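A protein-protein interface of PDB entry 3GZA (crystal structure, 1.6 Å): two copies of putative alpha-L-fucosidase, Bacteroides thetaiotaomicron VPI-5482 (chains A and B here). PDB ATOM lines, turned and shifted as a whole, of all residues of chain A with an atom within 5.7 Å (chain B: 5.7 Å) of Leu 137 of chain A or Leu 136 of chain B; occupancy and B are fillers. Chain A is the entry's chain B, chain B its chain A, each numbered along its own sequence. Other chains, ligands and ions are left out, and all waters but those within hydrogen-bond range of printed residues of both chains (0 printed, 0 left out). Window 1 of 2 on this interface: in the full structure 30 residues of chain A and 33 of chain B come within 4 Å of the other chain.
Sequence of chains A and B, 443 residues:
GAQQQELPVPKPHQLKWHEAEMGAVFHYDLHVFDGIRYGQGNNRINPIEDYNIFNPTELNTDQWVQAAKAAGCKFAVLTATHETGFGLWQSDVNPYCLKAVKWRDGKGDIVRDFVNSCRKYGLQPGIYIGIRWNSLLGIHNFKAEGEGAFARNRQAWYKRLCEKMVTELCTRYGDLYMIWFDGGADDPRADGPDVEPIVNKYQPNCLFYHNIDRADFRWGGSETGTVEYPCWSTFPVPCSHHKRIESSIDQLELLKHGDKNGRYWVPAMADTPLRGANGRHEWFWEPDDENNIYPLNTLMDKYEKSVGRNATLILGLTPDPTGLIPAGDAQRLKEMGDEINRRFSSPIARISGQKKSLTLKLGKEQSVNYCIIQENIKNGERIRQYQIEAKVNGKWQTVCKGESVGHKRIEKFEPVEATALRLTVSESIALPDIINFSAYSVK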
ATOM      1  N   THR A  84      25.498 -27.796 -25.434  1.00  0.00           N
ATOM      2  CA  THR A  84      24.158 -27.180 -25.414  1.00  0.00           C
ATOM      3  C   THR A  84      23.159 -27.962 -24.549  1.00  0.00           C
ATOM      4  O   THR A  84      22.110 -27.408 -24.155  1.00  0.00           O
ATOM      5  CB  THR A  84      23.545 -27.054 -26.827  1.00  0.00           C
ATOM      6  OG1 THR A  84      23.248 -28.361 -27.354  1.00  0.00           O
ATOM      7  CG2 THR A  84      24.469 -26.281 -27.786  1.00  0.00           C
ATOM      8  N   PRO A  95      14.856 -34.649 -22.768  1.00  0.00           N
ATOM      9  CA  PRO A  95      13.853 -34.334 -23.767  1.00  0.00           C
ATOM     10  C   PRO A  95      14.403 -33.469 -24.902  1.00  0.00           C
ATOM     11  O   PRO A  95      13.824 -33.374 -25.991  1.00  0.00           O
ATOM     12  CB  PRO A  95      12.808 -33.549 -22.954  1.00  0.00           C
ATOM     13  CG  PRO A  95      13.631 -32.828 -21.914  1.00  0.00           C
ATOM     14  CD  PRO A  95      14.676 -33.882 -21.531  1.00  0.00           C
ATOM     15  N   ASN A 134      25.657 -27.590 -19.749  1.00  0.00           N
ATOM     16  CA  ASN A 134      24.361 -27.769 -20.411  1.00  0.00           C
ATOM     17  C   ASN A 134      23.664 -26.413 -20.444  1.00  0.00           C
ATOM     18  O   ASN A 134      23.200 -25.913 -19.445  1.00  0.00           O
ATOM     19  CB  ASN A 134      23.550 -28.830 -19.678  1.00  0.00           C
ATOM     20  CG  ASN A 134      22.225 -29.110 -20.352  1.00  0.00           C
ATOM     21  OD1 ASN A 134      21.502 -28.172 -20.753  1.00  0.00           O
ATOM     22  ND2 ASN A 134      21.860 -30.384 -20.433  1.00  0.00           N
ATOM     23  N   SER A 135      23.668 -25.758 -21.598  1.00  0.00           N
ATOM     24  CA  SER A 135      23.185 -24.395 -21.655  1.00  0.00           C
ATOM     25  C   SER A 135      21.682 -24.345 -21.497  1.00  0.00           C
ATOM     26  O   SER A 135      21.181 -23.410 -20.908  1.00  0.00           O
ATOM     27  CB  SER A 135      23.623 -23.676 -22.937  1.00  0.00           C
ATOM     28  OG  SER A 135      23.115 -24.234 -24.081  1.00  0.00           O
ATOM     29  N   LEU A 136      20.966 -25.331 -22.018  1.00  0.00           N
ATOM     30  CA  LEU A 136      19.505 -25.314 -21.838  1.00  0.00           C
ATOM     31  C   LEU A 136      19.130 -25.228 -20.371  1.00  0.00           C
ATOM     32  O   LEU A 136      18.249 -24.494 -19.943  1.00  0.00           O
ATOM     33  CB  LEU A 136      18.856 -26.562 -22.452  1.00  0.00           C
ATOM     34  CG  LEU A 136      17.341 -26.769 -22.207  1.00  0.00           C
ATOM     35  CD1 LEU A 136      16.572 -25.639 -22.903  1.00  0.00           C
ATOM     36  CD2 LEU A 136      16.903 -28.130 -22.655  1.00  0.00           C
ATOM     37  N   LEU A 137      19.826 -26.036 -19.590  1.00  0.00           N
ATOM     38  CA  LEU A 137      19.555 -26.179 -18.162  1.00  0.00           C
ATOM     39  C   LEU A 137      20.362 -25.279 -17.243  1.00  0.00           C
ATOM     40  O   LEU A 137      20.143 -25.278 -16.025  1.00  0.00           O
ATOM     41  CB  LEU A 137      19.761 -27.645 -17.735  1.00  0.00           C
ATOM     42  CG  LEU A 137      18.881 -28.697 -18.410  1.00  0.00           C
ATOM     43  CD1 LEU A 137      19.207 -30.156 -17.988  1.00  0.00           C
ATOM     44  CD2 LEU A 137      17.361 -28.363 -18.197  1.00  0.00           C
ATOM     45  N   GLY A 138      21.242 -24.469 -17.804  1.00  0.00           N
ATOM     46  CA  GLY A 138      22.033 -23.556 -17.042  1.00  0.00           C
ATOM     47  C   GLY A 138      23.080 -24.201 -16.138  1.00  0.00           C
ATOM     48  O   GLY A 138      23.369 -23.677 -15.067  1.00  0.00           O
ATOM     49  N   ILE A 139      23.636 -25.316 -16.574  1.00  0.00           N
ATOM     50  CA  ILE A 139      24.616 -26.060 -15.773  1.00  0.00           C
ATOM     51  C   ILE A 139      26.042 -25.642 -16.155  1.00  0.00           C
ATOM     52  O   ILE A 139      26.371 -25.589 -17.339  1.00  0.00           O
ATOM     53  CB  ILE A 139      24.386 -27.559 -15.949  1.00  0.00           C
ATOM     54  CG1 ILE A 139      23.021 -27.950 -15.351  1.00  0.00           C
ATOM     55  CG2 ILE A 139      25.565 -28.370 -15.311  1.00  0.00           C
ATOM     56  CD1 ILE A 139      22.920 -27.901 -13.813  1.00  0.00           C
ATOM     57  N   PHE A 150      16.239 -24.744  -4.357  1.00  0.00           N
ATOM     58  CA  PHE A 150      15.921 -25.000  -5.748  1.00  0.00           C
ATOM     59  C   PHE A 150      17.152 -25.345  -6.562  1.00  0.00           C
ATOM     60  O   PHE A 150      17.178 -26.344  -7.265  1.00  0.00           O
ATOM     61  CB  PHE A 150      15.120 -23.788  -6.295  1.00  0.00           C
ATOM     62  CG  PHE A 150      14.568 -23.951  -7.710  1.00  0.00           C
ATOM     63  CD1 PHE A 150      14.325 -25.178  -8.327  1.00  0.00           C
ATOM     64  CD2 PHE A 150      14.133 -22.825  -8.356  1.00  0.00           C
ATOM     65  CE1 PHE A 150      13.734 -25.276  -9.586  1.00  0.00           C
ATOM     66  CE2 PHE A 150      13.554 -22.906  -9.624  1.00  0.00           C
ATOM     67  CZ  PHE A 150      13.380 -24.118 -10.236  1.00  0.00           C
ATOM     68  N   ARG A 154      18.013 -28.929  -8.377  1.00  0.00           N
ATOM     69  CA  ARG A 154      18.305 -29.019  -9.788  1.00  0.00           C
ATOM     70  C   ARG A 154      19.693 -29.636 -10.047  1.00  0.00           C
ATOM     71  O   ARG A 154      19.859 -30.386 -11.007  1.00  0.00           O
ATOM     72  CB  ARG A 154      18.205 -27.638 -10.468  1.00  0.00           C
ATOM     73  CG  ARG A 154      16.792 -27.037 -10.504  1.00  0.00           C
ATOM     74  CD  ARG A 154      16.650 -26.042 -11.664  1.00  0.00           C
ATOM     75  NE  ARG A 154      17.792 -25.113 -11.708  1.00  0.00           N
ATOM     76  CZ  ARG A 154      18.038 -24.121 -10.836  1.00  0.00           C
ATOM     77  NH1 ARG A 154      17.254 -23.833  -9.800  1.00  0.00           N
ATOM     78  NH2 ARG A 154      19.100 -23.386 -11.009  1.00  0.00           N
ATOM     79  N   TRP A 157      19.351 -33.333  -9.361  1.00  0.00           N
ATOM     80  CA  TRP A 157      18.570 -33.893 -10.433  1.00  0.00           C
ATOM     81  C   TRP A 157      19.431 -34.030 -11.694  1.00  0.00           C
ATOM     82  O   TRP A 157      19.357 -35.058 -12.400  1.00  0.00           O
ATOM     83  CB  TRP A 157      17.327 -33.021 -10.656  1.00  0.00           C
ATOM     84  CG  TRP A 157      16.471 -33.419 -11.795  1.00  0.00           C
ATOM     85  CD1 TRP A 157      15.356 -34.192 -11.730  1.00  0.00           C
ATOM     86  CD2 TRP A 157      16.654 -33.078 -13.162  1.00  0.00           C
ATOM     87  NE1 TRP A 157      14.835 -34.352 -12.982  1.00  0.00           N
ATOM     88  CE2 TRP A 157      15.609 -33.692 -13.885  1.00  0.00           C
ATOM     89  CE3 TRP A 157      17.618 -32.335 -13.867  1.00  0.00           C
ATOM     90  CZ2 TRP A 157      15.477 -33.579 -15.261  1.00  0.00           C
ATOM     91  CZ3 TRP A 157      17.472 -32.238 -15.235  1.00  0.00           C
ATOM     92  CH2 TRP A 157      16.410 -32.855 -15.920  1.00  0.00           C
ATOM     93  N   TYR A 158      20.268 -33.026 -11.969  1.00  0.00           N
ATOM     94  CA  TYR A 158      21.113 -33.069 -13.158  1.00  0.00           C
ATOM     95  C   TYR A 158      22.116 -34.219 -13.068  1.00  0.00           C
ATOM     96  O   TYR A 158      22.370 -34.891 -14.074  1.00  0.00           O
ATOM     97  CB  TYR A 158      21.835 -31.730 -13.362  1.00  0.00           C
ATOM     98  CG  TYR A 158      22.706 -31.752 -14.592  1.00  0.00           C
ATOM     99  CD1 TYR A 158      22.152 -31.735 -15.874  1.00  0.00           C
ATOM    100  CD2 TYR A 158      24.079 -31.817 -14.503  1.00  0.00           C
ATOM    101  CE1 TYR A 158      22.926 -31.780 -16.982  1.00  0.00           C
ATOM    102  CE2 TYR A 158      24.856 -31.868 -15.621  1.00  0.00           C
ATOM    103  CZ  TYR A 158      24.297 -31.856 -16.855  1.00  0.00           C
ATOM    104  OH  TYR A 158      25.039 -31.873 -18.049  1.00  0.00           O
ATOM    105  N   LEU A 161      20.290 -37.134 -14.111  1.00  0.00           N
ATOM    106  CA  LEU A 161      20.062 -37.096 -15.539  1.00  0.00           C
ATOM    107  C   LEU A 161      21.297 -37.644 -16.250  1.00  0.00           C
ATOM    108  O   LEU A 161      21.174 -38.462 -17.178  1.00  0.00           O
ATOM    109  CB  LEU A 161      19.798 -35.647 -16.027  1.00  0.00           C
ATOM    110  CG  LEU A 161      19.683 -35.463 -17.520  1.00  0.00           C
ATOM    111  CD1 LEU A 161      18.502 -36.224 -18.073  1.00  0.00           C
ATOM    112  CD2 LEU A 161      19.624 -34.013 -17.980  1.00  0.00           C
ATOM    113  N   PRO B  47      12.482 -30.778 -10.023  1.00  0.00           N
ATOM    114  CA  PRO B  47      12.130 -31.230 -11.341  1.00  0.00           C
ATOM    115  C   PRO B  47      11.652 -32.709 -11.319  1.00  0.00           C
ATOM    116  O   PRO B  47      12.098 -33.526 -10.501  1.00  0.00           O
ATOM    117  CB  PRO B  47      13.444 -31.079 -12.124  1.00  0.00           C
ATOM    118  CG  PRO B  47      14.214 -30.062 -11.392  1.00  0.00           C
ATOM    119  CD  PRO B  47      13.869 -30.287  -9.945  1.00  0.00           C
ATOM    120  N   GLU B  83       3.675 -25.779 -13.595  1.00  0.00           N
ATOM    121  CA  GLU B  83       4.877 -25.536 -12.836  1.00  0.00           C
ATOM    122  C   GLU B  83       6.069 -26.410 -13.189  1.00  0.00           C
ATOM    123  O   GLU B  83       7.187 -26.025 -12.912  1.00  0.00           O
ATOM    124  CB  GLU B  83       4.602 -25.745 -11.340  1.00  0.00           C
ATOM    125  CG  GLU B  83       3.647 -24.700 -10.724  1.00  0.00           C
ATOM    126  CD  GLU B  83       3.070 -25.128  -9.385  1.00  0.00           C
ATOM    127  OE1 GLU B  83       3.086 -26.350  -9.056  1.00  0.00           O
ATOM    128  OE2 GLU B  83       2.519 -24.262  -8.701  1.00  0.00           O
ATOM    129  N   THR B  84       5.867 -27.571 -13.802  1.00  0.00           N
ATOM    130  CA  THR B  84       7.012 -28.465 -14.059  1.00  0.00           C
ATOM    131  C   THR B  84       7.831 -28.010 -15.251  1.00  0.00           C
ATOM    132  O   THR B  84       8.966 -28.421 -15.405  1.00  0.00           O
ATOM    133  CB  THR B  84       6.597 -29.915 -14.313  1.00  0.00           C
ATOM    134  OG1 THR B  84       5.922 -30.017 -15.582  1.00  0.00           O
ATOM    135  CG2 THR B  84       5.725 -30.482 -13.157  1.00  0.00           C
ATOM    136  N   GLY B  85       7.204 -27.201 -16.092  1.00  0.00           N
ATOM    137  CA  GLY B  85       7.737 -26.800 -17.365  1.00  0.00           C
ATOM    138  C   GLY B  85       7.243 -27.648 -18.518  1.00  0.00           C
ATOM    139  O   GLY B  85       7.515 -27.263 -19.655  1.00  0.00           O
ATOM    140  N   TYR B  96      10.447 -29.920 -23.770  1.00  0.00           N
ATOM    141  CA  TYR B  96       9.846 -30.644 -22.652  1.00  0.00           C
ATOM    142  C   TYR B  96       8.344 -30.624 -22.803  1.00  0.00           C
ATOM    143  O   TYR B  96       7.619 -29.844 -22.175  1.00  0.00           O
ATOM    144  CB  TYR B  96      10.219 -29.945 -21.352  1.00  0.00           C
ATOM    145  CG  TYR B  96      10.066 -30.724 -20.083  1.00  0.00           C
ATOM    146  CD1 TYR B  96      10.491 -32.043 -19.976  1.00  0.00           C
ATOM    147  CD2 TYR B  96       9.583 -30.122 -18.929  1.00  0.00           C
ATOM    148  CE1 TYR B  96      10.447 -32.734 -18.764  1.00  0.00           C
ATOM    149  CE2 TYR B  96       9.522 -30.833 -17.733  1.00  0.00           C
ATOM    150  CZ  TYR B  96       9.954 -32.117 -17.660  1.00  0.00           C
ATOM    151  OH  TYR B  96       9.995 -32.775 -16.438  1.00  0.00           O
ATOM    152  N   ASN B 134       8.981 -22.816 -13.327  1.00  0.00           N
ATOM    153  CA  ASN B 134       9.395 -23.872 -14.253  1.00  0.00           C
ATOM    154  C   ASN B 134      10.516 -24.605 -13.570  1.00  0.00           C
ATOM    155  O   ASN B 134      11.643 -24.094 -13.449  1.00  0.00           O
ATOM    156  CB  ASN B 134       9.834 -23.269 -15.578  1.00  0.00           C
ATOM    157  CG  ASN B 134      10.189 -24.314 -16.601  1.00  0.00           C
ATOM    158  OD1 ASN B 134      10.774 -25.383 -16.251  1.00  0.00           O
ATOM    159  ND2 ASN B 134       9.819 -24.049 -17.898  1.00  0.00           N
ATOM    160  N   SER B 135      10.170 -25.747 -12.984  1.00  0.00           N
ATOM    161  CA  SER B 135      11.144 -26.482 -12.200  1.00  0.00           C
ATOM    162  C   SER B 135      12.302 -26.992 -13.047  1.00  0.00           C
ATOM    163  O   SER B 135      13.442 -26.947 -12.624  1.00  0.00           O
ATOM    164  CB  SER B 135      10.502 -27.627 -11.446  1.00  0.00           C
ATOM    165  OG  SER B 135       9.944 -28.578 -12.315  1.00  0.00           O
ATOM    166  N   LEU B 136      12.005 -27.429 -14.254  1.00  0.00           N
ATOM    167  CA  LEU B 136      13.085 -27.970 -15.104  1.00  0.00           C
ATOM    168  C   LEU B 136      14.117 -26.907 -15.411  1.00  0.00           C
ATOM    169  O   LEU B 136      15.324 -27.178 -15.346  1.00  0.00           O
ATOM    170  CB  LEU B 136      12.524 -28.490 -16.447  1.00  0.00           C
ATOM    171  CG  LEU B 136      13.597 -29.105 -17.336  1.00  0.00           C
ATOM    172  CD1 LEU B 136      14.164 -30.443 -16.767  1.00  0.00           C
ATOM    173  CD2 LEU B 136      12.974 -29.207 -18.757  1.00  0.00           C
ATOM    174  N   LEU B 137      13.652 -25.725 -15.840  1.00  0.00           N
ATOM    175  CA  LEU B 137      14.488 -24.650 -16.333  1.00  0.00           C
ATOM    176  C   LEU B 137      15.003 -23.690 -15.301  1.00  0.00           C
ATOM    177  O   LEU B 137      15.766 -22.811 -15.626  1.00  0.00           O
ATOM    178  CB  LEU B 137      13.792 -23.877 -17.445  1.00  0.00           C
ATOM    179  CG  LEU B 137      13.399 -24.713 -18.672  1.00  0.00           C
ATOM    180  CD1 LEU B 137      12.798 -23.777 -19.692  1.00  0.00           C
ATOM    181  CD2 LEU B 137      14.614 -25.476 -19.280  1.00  0.00           C
ATOM    182  N   GLY B 138      14.631 -23.879 -14.042  1.00  0.00           N
ATOM    183  CA  GLY B 138      15.188 -23.032 -13.020  1.00  0.00           C
ATOM    184  C   GLY B 138      14.544 -21.654 -12.941  1.00  0.00           C
ATOM    185  O   GLY B 138      15.252 -20.681 -12.678  1.00  0.00           O
ATOM    186  N   ARG B 154      20.007 -15.249 -19.496  1.00  0.00           N
ATOM    187  CA  ARG B 154      19.051 -16.329 -19.370  1.00  0.00           C
ATOM    188  C   ARG B 154      17.638 -15.779 -19.216  1.00  0.00           C
ATOM    189  O   ARG B 154      16.676 -16.321 -19.788  1.00  0.00           O
ATOM    190  CB  ARG B 154      19.463 -17.267 -18.228  1.00  0.00           C
ATOM    191  CG  ARG B 154      18.589 -18.463 -18.189  1.00  0.00           C
ATOM    192  CD  ARG B 154      19.138 -19.529 -17.209  1.00  0.00           C
ATOM    193  NE  ARG B 154      18.337 -20.742 -17.148  1.00  0.00           N
ATOM    194  CZ  ARG B 154      18.412 -21.742 -18.021  1.00  0.00           C
ATOM    195  NH1 ARG B 154      19.249 -21.703 -19.045  1.00  0.00           N
ATOM    196  NH2 ARG B 154      17.636 -22.790 -17.841  1.00  0.00           N
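The guanidinium group of Arg 154 of chain B sits at hydrogen-bond distance from the backbone carbonyl oxygen of Ser 135 of chain A (3.2 Å). The guanidinium group of Arg 154 of chain B is in hydrogen-bond range of the backbone carbonyl oxygen of Leu 136 of chain A, 2.8 Å away.
O of Glu 83 of chain B lies within hydrogen-bond range of N of Ser 135 of chain B. OG of Ser 135 of chain B is in hydrogen-bond range of O of Thr 84 of chain B, 3.2 Å away. O of Leu 137 of chain B is in hydrogen-bond range of NH2 of Arg 154 of chain B (2.9 Å). The backbone carbonyl oxygen of Thr 84 of chain A lies within hydrogen-bond range of the side-chain hydroxyl of Ser 135 of chain A, 3.3 Å away. The backbone NH (N) of Leu 136 of chain A is in hydrogen-bond range of the backbone carbonyl oxygen (O) of Thr 84 of chain A (3.2 Å). OD1 of Asn 134 of chain A is in hydrogen-bond range of N of Leu 137 of chain A (3.0 Å).
Among the printed residues, merely in contact across the chains: Pro 95 of chain A with Tyr 96 of chain B, Leu 136 of chain A with Leu 137 of chain B, Leu 137 of chain A with Leu 136 of chain B, Leu 137 of chain A with Arg 154 of chain B, Gly 138 of chain A with Arg 154 of chain B, Phe 150 of chain A with Asn 134 of chain B, Phe 150 of chain A with Ser 135 of chain B, Phe 150 of chain A with Gly 138 of chain B, Arg 154 of chain A with Ser 135 of chain B, Arg 154 of chain A with Gly 138 of chain B, Trp 157 of chain A with Pro 47 of chain B and Trp 157 of chain A with Leu 136 of chain B.
Leu 137 of chain A touches two residues of chain B. Of the printed residues of chain A, Leu 136 of chain B touches Leu 137 (3.7 Å) and Trp 157 (3.4 Å). Of the printed residues of chain B, Arg 154 of chain A touches Ser 135 and Gly 138. Printed residues of chain A within 4 Å of Ser 135 of chain B: Phe 150 and Arg 154. Of the printed residues of chain B, Pro 95 of chain A touches Tyr 96 (3.8 Å). Thr 84 of chain B touches none of the printed residues of chain A. The nearest printed residue of chain B that does not touch Gly 138 of chain A is Leu 137 of chain B (6.1 Å).
Hydrophobic or aromatic side chains of chain B that line the printed part of chain A: Pro 47, Tyr 96, Leu 136 and Leu 137. Of the 13 printed residues of chain A, 8 touch a printed residue of chain B. Hydrophobic or aromatic side chains of chain A within 4 Å of the printed part of chain B: Pro 95, Leu 137, Phe 150 and Trp 157. Along chain A the printed residues that touch a printed residue of chain B span positions 95 to 157. Among the printed residues, no Asp or Glu carboxylate lies within 4 Å of a Lys or Arg side-chain nitrogen of the other chain.
Ser 135 of chain A touches Arg 154 of chain B, and with the chains exchanged Arg 154 of chain A touches Ser 135 of chain B. Leu 136 of chain A touches Arg 154 of chain B, but with the chains exchanged Arg 154 of chain A does not touch Leu 136 of chain B (4.1 Å). Leu 137 of chain A touches Arg 154 of chain B, but with the chains exchanged Arg 154 of chain A does not touch Leu 137 of chain B (4.6 Å). Gly 138 of chain A touches Arg 154 of chain B, and with the chains exchanged Arg 154 of chain A touches Gly 138 of chain B. 7 positions are printed for both chains.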
